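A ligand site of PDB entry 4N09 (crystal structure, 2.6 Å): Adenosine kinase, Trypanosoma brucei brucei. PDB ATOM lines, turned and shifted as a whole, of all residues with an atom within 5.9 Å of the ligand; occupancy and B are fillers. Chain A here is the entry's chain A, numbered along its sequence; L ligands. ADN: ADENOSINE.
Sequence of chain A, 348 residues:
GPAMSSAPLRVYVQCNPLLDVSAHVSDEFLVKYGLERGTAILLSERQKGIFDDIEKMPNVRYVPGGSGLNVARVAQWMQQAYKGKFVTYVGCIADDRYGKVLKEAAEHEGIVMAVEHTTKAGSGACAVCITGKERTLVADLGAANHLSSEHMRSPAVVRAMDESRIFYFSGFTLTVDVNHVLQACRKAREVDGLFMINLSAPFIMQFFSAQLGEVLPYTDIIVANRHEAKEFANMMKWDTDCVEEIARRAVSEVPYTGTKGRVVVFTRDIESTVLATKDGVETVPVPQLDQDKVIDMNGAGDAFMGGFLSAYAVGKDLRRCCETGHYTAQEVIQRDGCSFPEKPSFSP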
ATOM      1  N   CYS A  15     -30.054 -13.624  24.321  1.00  0.00           N
ATOM      2  CA  CYS A  15     -28.806 -13.677  23.581  1.00  0.00           C
ATOM      3  C   CYS A  15     -28.376 -15.109  23.403  1.00  0.00           C
ATOM      4  O   CYS A  15     -29.129 -16.026  23.709  1.00  0.00           O
ATOM      5  CB  CYS A  15     -27.730 -12.869  24.332  1.00  0.00           C
ATOM      6  SG  CYS A  15     -26.264 -12.442  23.334  1.00  0.00           S
ATOM      7  N   ASN A  16     -27.150 -15.292  22.933  1.00  0.00           N
ATOM      8  CA  ASN A  16     -26.549 -16.599  22.733  1.00  0.00           C
ATOM      9  C   ASN A  16     -25.604 -16.958  23.855  1.00  0.00           C
ATOM     10  O   ASN A  16     -24.590 -16.303  24.014  1.00  0.00           O
ATOM     11  CB  ASN A  16     -25.778 -16.550  21.438  1.00  0.00           C
ATOM     12  CG  ASN A  16     -26.631 -16.124  20.275  1.00  0.00           C
ATOM     13  OD1 ASN A  16     -27.827 -16.417  20.239  1.00  0.00           O
ATOM     14  ND2 ASN A  16     -26.035 -15.439  19.328  1.00  0.00           N
ATOM     15  N   PRO A  17     -25.947 -17.944  24.691  1.00  0.00           N
ATOM     16  CA  PRO A  17     -25.057 -18.250  25.813  1.00  0.00           C
ATOM     17  C   PRO A  17     -23.862 -19.064  25.328  1.00  0.00           C
ATOM     18  O   PRO A  17     -24.065 -20.100  24.703  1.00  0.00           O
ATOM     19  CB  PRO A  17     -25.941 -19.051  26.767  1.00  0.00           C
ATOM     20  CG  PRO A  17     -27.019 -19.614  25.916  1.00  0.00           C
ATOM     21  CD  PRO A  17     -27.180 -18.745  24.713  1.00  0.00           C
ATOM     22  N   LEU A  18     -22.655 -18.570  25.547  1.00  0.00           N
ATOM     23  CA  LEU A  18     -21.433 -19.172  25.026  1.00  0.00           C
ATOM     24  C   LEU A  18     -20.413 -19.276  26.101  1.00  0.00           C
ATOM     25  O   LEU A  18     -20.343 -18.416  26.987  1.00  0.00           O
ATOM     26  CB  LEU A  18     -20.811 -18.314  23.941  1.00  0.00           C
ATOM     27  CG  LEU A  18     -21.708 -17.904  22.778  1.00  0.00           C
ATOM     28  CD1 LEU A  18     -20.918 -17.000  21.838  1.00  0.00           C
ATOM     29  CD2 LEU A  18     -22.253 -19.107  22.051  1.00  0.00           C
ATOM     30  N   LEU A  19     -19.629 -20.346  26.051  1.00  0.00           N
ATOM     31  CA  LEU A  19     -18.525 -20.511  26.950  1.00  0.00           C
ATOM     32  C   LEU A  19     -17.303 -19.941  26.304  1.00  0.00           C
ATOM     33  O   LEU A  19     -16.953 -20.338  25.201  1.00  0.00           O
ATOM     34  CB  LEU A  19     -18.294 -21.982  27.254  1.00  0.00           C
ATOM     35  CG  LEU A  19     -17.284 -22.125  28.392  1.00  0.00           C
ATOM     36  CD1 LEU A  19     -17.986 -22.445  29.718  1.00  0.00           C
ATOM     37  CD2 LEU A  19     -16.262 -23.186  28.038  1.00  0.00           C
ATOM     38  N   ASP A  20     -16.640 -19.028  27.000  1.00  0.00           N
ATOM     39  CA  ASP A  20     -15.434 -18.408  26.479  1.00  0.00           C
ATOM     40  C   ASP A  20     -14.215 -19.260  26.793  1.00  0.00           C
ATOM     41  O   ASP A  20     -13.911 -19.572  27.954  1.00  0.00           O
ATOM     42  CB  ASP A  20     -15.243 -16.988  27.039  1.00  0.00           C
ATOM     43  CG  ASP A  20     -16.208 -15.979  26.445  1.00  0.00           C
ATOM     44  OD1 ASP A  20     -16.856 -16.270  25.421  1.00  0.00           O
ATOM     45  OD2 ASP A  20     -16.304 -14.852  26.990  1.00  0.00           O
ATOM     46  N   ALA A  40     -14.988  -9.414  16.290  1.00  0.00           N
ATOM     47  CA  ALA A  40     -15.726 -10.641  16.523  1.00  0.00           C
ATOM     48  C   ALA A  40     -16.278 -11.130  15.195  1.00  0.00           C
ATOM     49  O   ALA A  40     -16.748 -10.333  14.405  1.00  0.00           O
ATOM     50  CB  ALA A  40     -16.861 -10.407  17.508  1.00  0.00           C
ATOM     51  N   ILE A  41     -16.199 -12.436  14.960  1.00  0.00           N
ATOM     52  CA  ILE A  41     -16.827 -13.087  13.782  1.00  0.00           C
ATOM     53  C   ILE A  41     -17.488 -14.374  14.221  1.00  0.00           C
ATOM     54  O   ILE A  41     -17.347 -14.801  15.367  1.00  0.00           O
ATOM     55  CB  ILE A  41     -15.801 -13.438  12.690  1.00  0.00           C
ATOM     56  CG1 ILE A  41     -14.737 -14.398  13.229  1.00  0.00           C
ATOM     57  CG2 ILE A  41     -15.129 -12.182  12.153  1.00  0.00           C
ATOM     58  CD1 ILE A  41     -13.930 -15.073  12.160  1.00  0.00           C
ATOM     59  N   LEU A  42     -18.220 -14.974  13.302  1.00  0.00           N
ATOM     60  CA  LEU A  42     -18.731 -16.316  13.505  1.00  0.00           C
ATOM     61  C   LEU A  42     -17.717 -17.293  12.919  1.00  0.00           C
ATOM     62  O   LEU A  42     -17.115 -17.030  11.864  1.00  0.00           O
ATOM     63  CB  LEU A  42     -20.096 -16.467  12.835  1.00  0.00           C
ATOM     64  CG  LEU A  42     -21.251 -15.598  13.351  1.00  0.00           C
ATOM     65  CD1 LEU A  42     -22.514 -15.888  12.541  1.00  0.00           C
ATOM     66  CD2 LEU A  42     -21.554 -15.849  14.840  1.00  0.00           C
ATOM     67  N   GLY A  65     -19.504 -17.032  29.271  1.00  0.00           N
ATOM     68  CA  GLY A  65     -19.531 -15.767  28.535  1.00  0.00           C
ATOM     69  C   GLY A  65     -20.861 -15.592  27.821  1.00  0.00           C
ATOM     70  O   GLY A  65     -21.899 -15.947  28.361  1.00  0.00           O
ATOM     71  N   GLY A  66     -20.808 -15.066  26.617  1.00  0.00           N
ATOM     72  CA  GLY A  66     -21.997 -14.653  25.900  1.00  0.00           C
ATOM     73  C   GLY A  66     -22.276 -13.192  26.206  1.00  0.00           C
ATOM     74  O   GLY A  66     -22.379 -12.803  27.378  1.00  0.00           O
ATOM     75  N   SER A  67     -22.434 -12.386  25.153  1.00  0.00           N
ATOM     76  CA  SER A  67     -22.575 -10.929  25.299  1.00  0.00           C
ATOM     77  C   SER A  67     -23.754 -10.536  26.162  1.00  0.00           C
ATOM     78  O   SER A  67     -23.614  -9.805  27.148  1.00  0.00           O
ATOM     79  CB  SER A  67     -22.747 -10.303  23.918  1.00  0.00           C
ATOM     80  OG  SER A  67     -22.862  -8.908  24.017  1.00  0.00           O
ATOM     81  N   GLY A  68     -24.927 -11.033  25.810  1.00  0.00           N
ATOM     82  CA  GLY A  68     -26.119 -10.713  26.590  1.00  0.00           C
ATOM     83  C   GLY A  68     -26.044 -11.228  28.020  1.00  0.00           C
ATOM     84  O   GLY A  68     -26.617 -10.647  28.935  1.00  0.00           O
ATOM     85  N   ASN A  70     -23.336 -11.666  29.818  1.00  0.00           N
ATOM     86  CA  ASN A  70     -22.517 -10.737  30.573  1.00  0.00           C
ATOM     87  C   ASN A  70     -23.319  -9.509  30.937  1.00  0.00           C
ATOM     88  O   ASN A  70     -23.205  -9.006  32.061  1.00  0.00           O
ATOM     89  CB  ASN A  70     -21.298 -10.258  29.765  1.00  0.00           C
ATOM     90  CG  ASN A  70     -20.330 -11.376  29.396  1.00  0.00           C
ATOM     91  OD1 ASN A  70     -20.218 -12.379  30.076  1.00  0.00           O
ATOM     92  ND2 ASN A  70     -19.651 -11.195  28.290  1.00  0.00           N
ATOM     93  N   CYS A 126     -16.950 -19.622  22.496  1.00  0.00           N
ATOM     94  CA  CYS A 126     -16.285 -18.543  21.794  1.00  0.00           C
ATOM     95  C   CYS A 126     -14.787 -18.603  22.035  1.00  0.00           C
ATOM     96  O   CYS A 126     -14.325 -18.631  23.186  1.00  0.00           O
ATOM     97  CB  CYS A 126     -16.819 -17.209  22.313  1.00  0.00           C
ATOM     98  SG  CYS A 126     -16.233 -15.797  21.345  1.00  0.00           S
ATOM     99  N   VAL A 128     -11.448 -16.929  22.417  1.00  0.00           N
ATOM    100  CA  VAL A 128     -11.004 -15.581  22.681  1.00  0.00           C
ATOM    101  C   VAL A 128      -9.507 -15.490  22.717  1.00  0.00           C
ATOM    102  O   VAL A 128      -8.839 -16.070  23.570  1.00  0.00           O
ATOM    103  CB  VAL A 128     -11.771 -14.842  23.831  1.00  0.00           C
ATOM    104  CG1 VAL A 128     -12.858 -15.689  24.493  1.00  0.00           C
ATOM    105  CG2 VAL A 128     -10.861 -14.176  24.842  1.00  0.00           C
ATOM    106  N   LEU A 137     -12.391 -12.372  18.777  1.00  0.00           N
ATOM    107  CA  LEU A 137     -13.400 -13.365  19.138  1.00  0.00           C
ATOM    108  C   LEU A 137     -13.898 -14.193  17.979  1.00  0.00           C
ATOM    109  O   LEU A 137     -14.206 -13.665  16.929  1.00  0.00           O
ATOM    110  CB  LEU A 137     -14.606 -12.666  19.760  1.00  0.00           C
ATOM    111  CG  LEU A 137     -14.243 -11.666  20.858  1.00  0.00           C
ATOM    112  CD1 LEU A 137     -15.484 -11.011  21.460  1.00  0.00           C
ATOM    113  CD2 LEU A 137     -13.426 -12.326  21.967  1.00  0.00           C
ATOM    114  N   VAL A 138     -13.998 -15.498  18.184  1.00  0.00           N
ATOM    115  CA  VAL A 138     -14.538 -16.363  17.157  1.00  0.00           C
ATOM    116  C   VAL A 138     -15.617 -17.220  17.776  1.00  0.00           C
ATOM    117  O   VAL A 138     -15.333 -18.069  18.610  1.00  0.00           O
ATOM    118  CB  VAL A 138     -13.446 -17.249  16.522  1.00  0.00           C
ATOM    119  CG1 VAL A 138     -14.039 -18.164  15.464  1.00  0.00           C
ATOM    120  CG2 VAL A 138     -12.367 -16.371  15.892  1.00  0.00           C
ATOM    121  N   ALA A 139     -16.866 -16.980  17.375  1.00  0.00           N
ATOM    122  CA  ALA A 139     -18.010 -17.559  18.084  1.00  0.00           C
ATOM    123  C   ALA A 139     -18.529 -18.752  17.345  1.00  0.00           C
ATOM    124  O   ALA A 139     -18.806 -18.673  16.150  1.00  0.00           O
ATOM    125  CB  ALA A 139     -19.109 -16.541  18.267  1.00  0.00           C
ATOM    126  N   LEU A 141     -21.583 -20.881  17.749  1.00  0.00           N
ATOM    127  CA  LEU A 141     -22.866 -20.867  18.441  1.00  0.00           C
ATOM    128  C   LEU A 141     -23.352 -22.232  18.888  1.00  0.00           C
ATOM    129  O   LEU A 141     -23.947 -22.365  19.956  1.00  0.00           O
ATOM    130  CB  LEU A 141     -23.910 -20.211  17.562  1.00  0.00           C
ATOM    131  CG  LEU A 141     -24.109 -18.710  17.709  1.00  0.00           C
ATOM    132  CD1 LEU A 141     -22.822 -17.944  17.864  1.00  0.00           C
ATOM    133  CD2 LEU A 141     -24.926 -18.156  16.555  1.00  0.00           C
ATOM    134  N   SER A 170     -29.438  -8.618  22.217  1.00  0.00           N
ATOM    135  CA  SER A 170     -28.201  -8.239  21.563  1.00  0.00           C
ATOM    136  C   SER A 170     -28.410  -8.368  20.062  1.00  0.00           C
ATOM    137  O   SER A 170     -29.244  -9.144  19.600  1.00  0.00           O
ATOM    138  CB  SER A 170     -27.050  -9.138  22.020  1.00  0.00           C
ATOM    139  OG  SER A 170     -27.131 -10.377  21.367  1.00  0.00           O
ATOM    140  N   PHE A 172     -26.398  -9.712  18.101  1.00  0.00           N
ATOM    141  CA  PHE A 172     -26.001 -11.052  17.816  1.00  0.00           C
ATOM    142  C   PHE A 172     -27.143 -12.048  17.664  1.00  0.00           C
ATOM    143  O   PHE A 172     -26.950 -13.086  17.031  1.00  0.00           O
ATOM    144  CB  PHE A 172     -25.094 -11.568  18.955  1.00  0.00           C
ATOM    145  CG  PHE A 172     -23.702 -10.988  18.953  1.00  0.00           C
ATOM    146  CD1 PHE A 172     -22.931 -10.968  17.805  1.00  0.00           C
ATOM    147  CD2 PHE A 172     -23.144 -10.548  20.136  1.00  0.00           C
ATOM    148  CE1 PHE A 172     -21.651 -10.461  17.819  1.00  0.00           C
ATOM    149  CE2 PHE A 172     -21.855 -10.041  20.171  1.00  0.00           C
ATOM    150  CZ  PHE A 172     -21.107 -10.004  19.009  1.00  0.00           C
ATOM    151  N   THR A 175     -28.571 -13.308  14.062  1.00  0.00           N
ATOM    152  CA  THR A 175     -28.030 -14.345  13.198  1.00  0.00           C
ATOM    153  C   THR A 175     -28.732 -15.653  13.429  1.00  0.00           C
ATOM    154  O   THR A 175     -28.557 -16.596  12.673  1.00  0.00           O
ATOM    155  CB  THR A 175     -26.515 -14.563  13.377  1.00  0.00           C
ATOM    156  OG1 THR A 175     -26.226 -15.319  14.572  1.00  0.00           O
ATOM    157  CG2 THR A 175     -25.767 -13.229  13.410  1.00  0.00           C
ATOM    158  N   PHE A 203     -20.234  -6.869  11.533  1.00  0.00           N
ATOM    159  CA  PHE A 203     -20.706  -7.865  10.592  1.00  0.00           C
ATOM    160  C   PHE A 203     -22.230  -7.988  10.563  1.00  0.00           C
ATOM    161  O   PHE A 203     -22.802  -8.380   9.563  1.00  0.00           O
ATOM    162  CB  PHE A 203     -20.000  -9.213  10.772  1.00  0.00           C
ATOM    163  CG  PHE A 203     -20.540 -10.057  11.874  1.00  0.00           C
ATOM    164  CD1 PHE A 203     -21.700 -10.774  11.726  1.00  0.00           C
ATOM    165  CD2 PHE A 203     -19.810 -10.198  13.026  1.00  0.00           C
ATOM    166  CE1 PHE A 203     -22.155 -11.600  12.736  1.00  0.00           C
ATOM    167  CE2 PHE A 203     -20.253 -11.015  14.055  1.00  0.00           C
ATOM    168  CZ  PHE A 203     -21.434 -11.725  13.902  1.00  0.00           C
ATOM    169  N   ASN A 298     -12.040  -6.089  26.681  1.00  0.00           N
ATOM    170  CA  ASN A 298     -13.100  -6.952  26.222  1.00  0.00           C
ATOM    171  C   ASN A 298     -14.275  -6.962  27.140  1.00  0.00           C
ATOM    172  O   ASN A 298     -14.111  -7.038  28.355  1.00  0.00           O
ATOM    173  CB  ASN A 298     -12.563  -8.365  26.143  1.00  0.00           C
ATOM    174  CG  ASN A 298     -13.536  -9.296  25.473  1.00  0.00           C
ATOM    175  OD1 ASN A 298     -13.880  -9.101  24.295  1.00  0.00           O
ATOM    176  ND2 ASN A 298     -13.980 -10.304  26.203  1.00  0.00           N
ATOM    177  N   GLY A 299     -15.461  -6.868  26.532  1.00  0.00           N
ATOM    178  CA  GLY A 299     -16.684  -6.811  27.291  1.00  0.00           C
ATOM    179  C   GLY A 299     -16.998  -5.460  27.901  1.00  0.00           C
ATOM    180  O   GLY A 299     -17.963  -5.345  28.627  1.00  0.00           O
ATOM    181  N   ALA A 300     -16.204  -4.426  27.612  1.00  0.00           N
ATOM    182  CA  ALA A 300     -16.503  -3.102  28.152  1.00  0.00           C
ATOM    183  C   ALA A 300     -17.912  -2.675  27.784  1.00  0.00           C
ATOM    184  O   ALA A 300     -18.633  -2.125  28.628  1.00  0.00           O
ATOM    185  CB  ALA A 300     -15.517  -2.080  27.654  1.00  0.00           C
ATOM    186  N   ASP A 302     -20.448  -4.644  26.970  1.00  0.00           N
ATOM    187  CA  ASP A 302     -21.404  -5.465  27.706  1.00  0.00           C
ATOM    188  C   ASP A 302     -21.567  -4.892  29.122  1.00  0.00           C
ATOM    189  O   ASP A 302     -22.663  -4.835  29.656  1.00  0.00           O
ATOM    190  CB  ASP A 302     -20.940  -6.906  27.812  1.00  0.00           C
ATOM    191  CG  ASP A 302     -20.861  -7.629  26.467  1.00  0.00           C
ATOM    192  OD1 ASP A 302     -21.529  -7.219  25.505  1.00  0.00           O
ATOM    193  OD2 ASP A 302     -20.131  -8.652  26.382  1.00  0.00           O
HETATM  194  O5' ADN L   1     -18.360  -8.891  24.694  1.00  0.00           O
HETATM  195  C5' ADN L   1     -17.589 -10.066  24.442  1.00  0.00           C
HETATM  196  C4' ADN L   1     -18.464 -11.279  24.511  1.00  0.00           C
HETATM  197  O4' ADN L   1     -19.019 -11.498  23.230  1.00  0.00           O
HETATM  198  C3' ADN L   1     -17.762 -12.570  24.835  1.00  0.00           C
HETATM  199  O3' ADN L   1     -18.083 -12.837  26.185  1.00  0.00           O
HETATM  200  C2' ADN L   1     -18.344 -13.612  23.885  1.00  0.00           C
HETATM  201  O2' ADN L   1     -18.833 -14.842  24.481  1.00  0.00           O
HETATM  202  C1' ADN L   1     -19.481 -12.835  23.254  1.00  0.00           C
HETATM  203  N9  ADN L   1     -19.817 -13.134  21.868  1.00  0.00           N
HETATM  204  C8  ADN L   1     -18.986 -13.024  20.817  1.00  0.00           C
HETATM  205  N7  ADN L   1     -19.592 -13.314  19.636  1.00  0.00           N
HETATM  206  C5  ADN L   1     -20.853 -13.602  20.003  1.00  0.00           C
HETATM  207  C6  ADN L   1     -22.039 -13.997  19.260  1.00  0.00           C
HETATM  208  N6  ADN L   1     -21.980 -14.123  17.932  1.00  0.00           N
HETATM  209  N1  ADN L   1     -23.140 -14.186  19.996  1.00  0.00           N
HETATM  210  C2  ADN L   1     -23.191 -14.027  21.340  1.00  0.00           C
HETATM  211  N3  ADN L   1     -22.139 -13.678  22.084  1.00  0.00           N
HETATM  212  C4  ADN L   1     -21.000 -13.453  21.453  1.00  0.00           C
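A nitrogen (N1) of the ligand is in hydrogen-bond range of the side-chain amide nitrogen of Asn 16 (3.2 Å). The side-chain carboxylate (OD2) of Asp 302 is in hydrogen-bond range of an oxygen (O5') of the ligand (2.5 Å). The backbone NH (N) of Ser 67 lies within hydrogen-bond range of a nitrogen (N3) of the ligand (3.3 Å). O2' of the ligand lies within hydrogen-bond range of OD1 of Asp 20 (2.6 Å). The side-chain amide nitrogen (ND2) of Asn 70 is in hydrogen-bond range of an oxygen (O3') of the ligand, at 3.1 Å. N of Gly 66 is in hydrogen-bond range of O2' of the ligand, at 2.9 Å.
The backbone NH (N) of Ala 139 sits at hydrogen-bond distance from the backbone carbonyl oxygen (O) of Ile 41 (3.0 Å). The side-chain sulfur (SG) of Cys 15 is in hydrogen-bond range of the side-chain hydroxyl (OG) of Ser 170, 3.0 Å away. The backbone NH of Gly 68 lies within hydrogen-bond range of the side-chain sulfur of Cys 15 (3.1 Å). The backbone carbonyl oxygen (O) of Phe 172 lies within hydrogen-bond range of the side-chain hydroxyl (OG1) of Thr 175, at 3.4 Å. The backbone carbonyl oxygen of Phe 172 lies within hydrogen-bond range of the side-chain amide nitrogen of Asn 16, at 3.4 Å. O of Leu 18 sits at hydrogen-bond distance from N of Gly 65 (2.8 Å). N of Cys 126 sits at hydrogen-bond distance from O of Leu 19 (2.8 Å). O of Leu 18 sits at hydrogen-bond distance from N of Gly 66.
Residues that only touch the ligand: Cys 15, Leu 18, Leu 42, Gly 65, Cys 126, Leu 137, Ala 139, Leu 141, Phe 172, Asn 298 and Gly 299.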
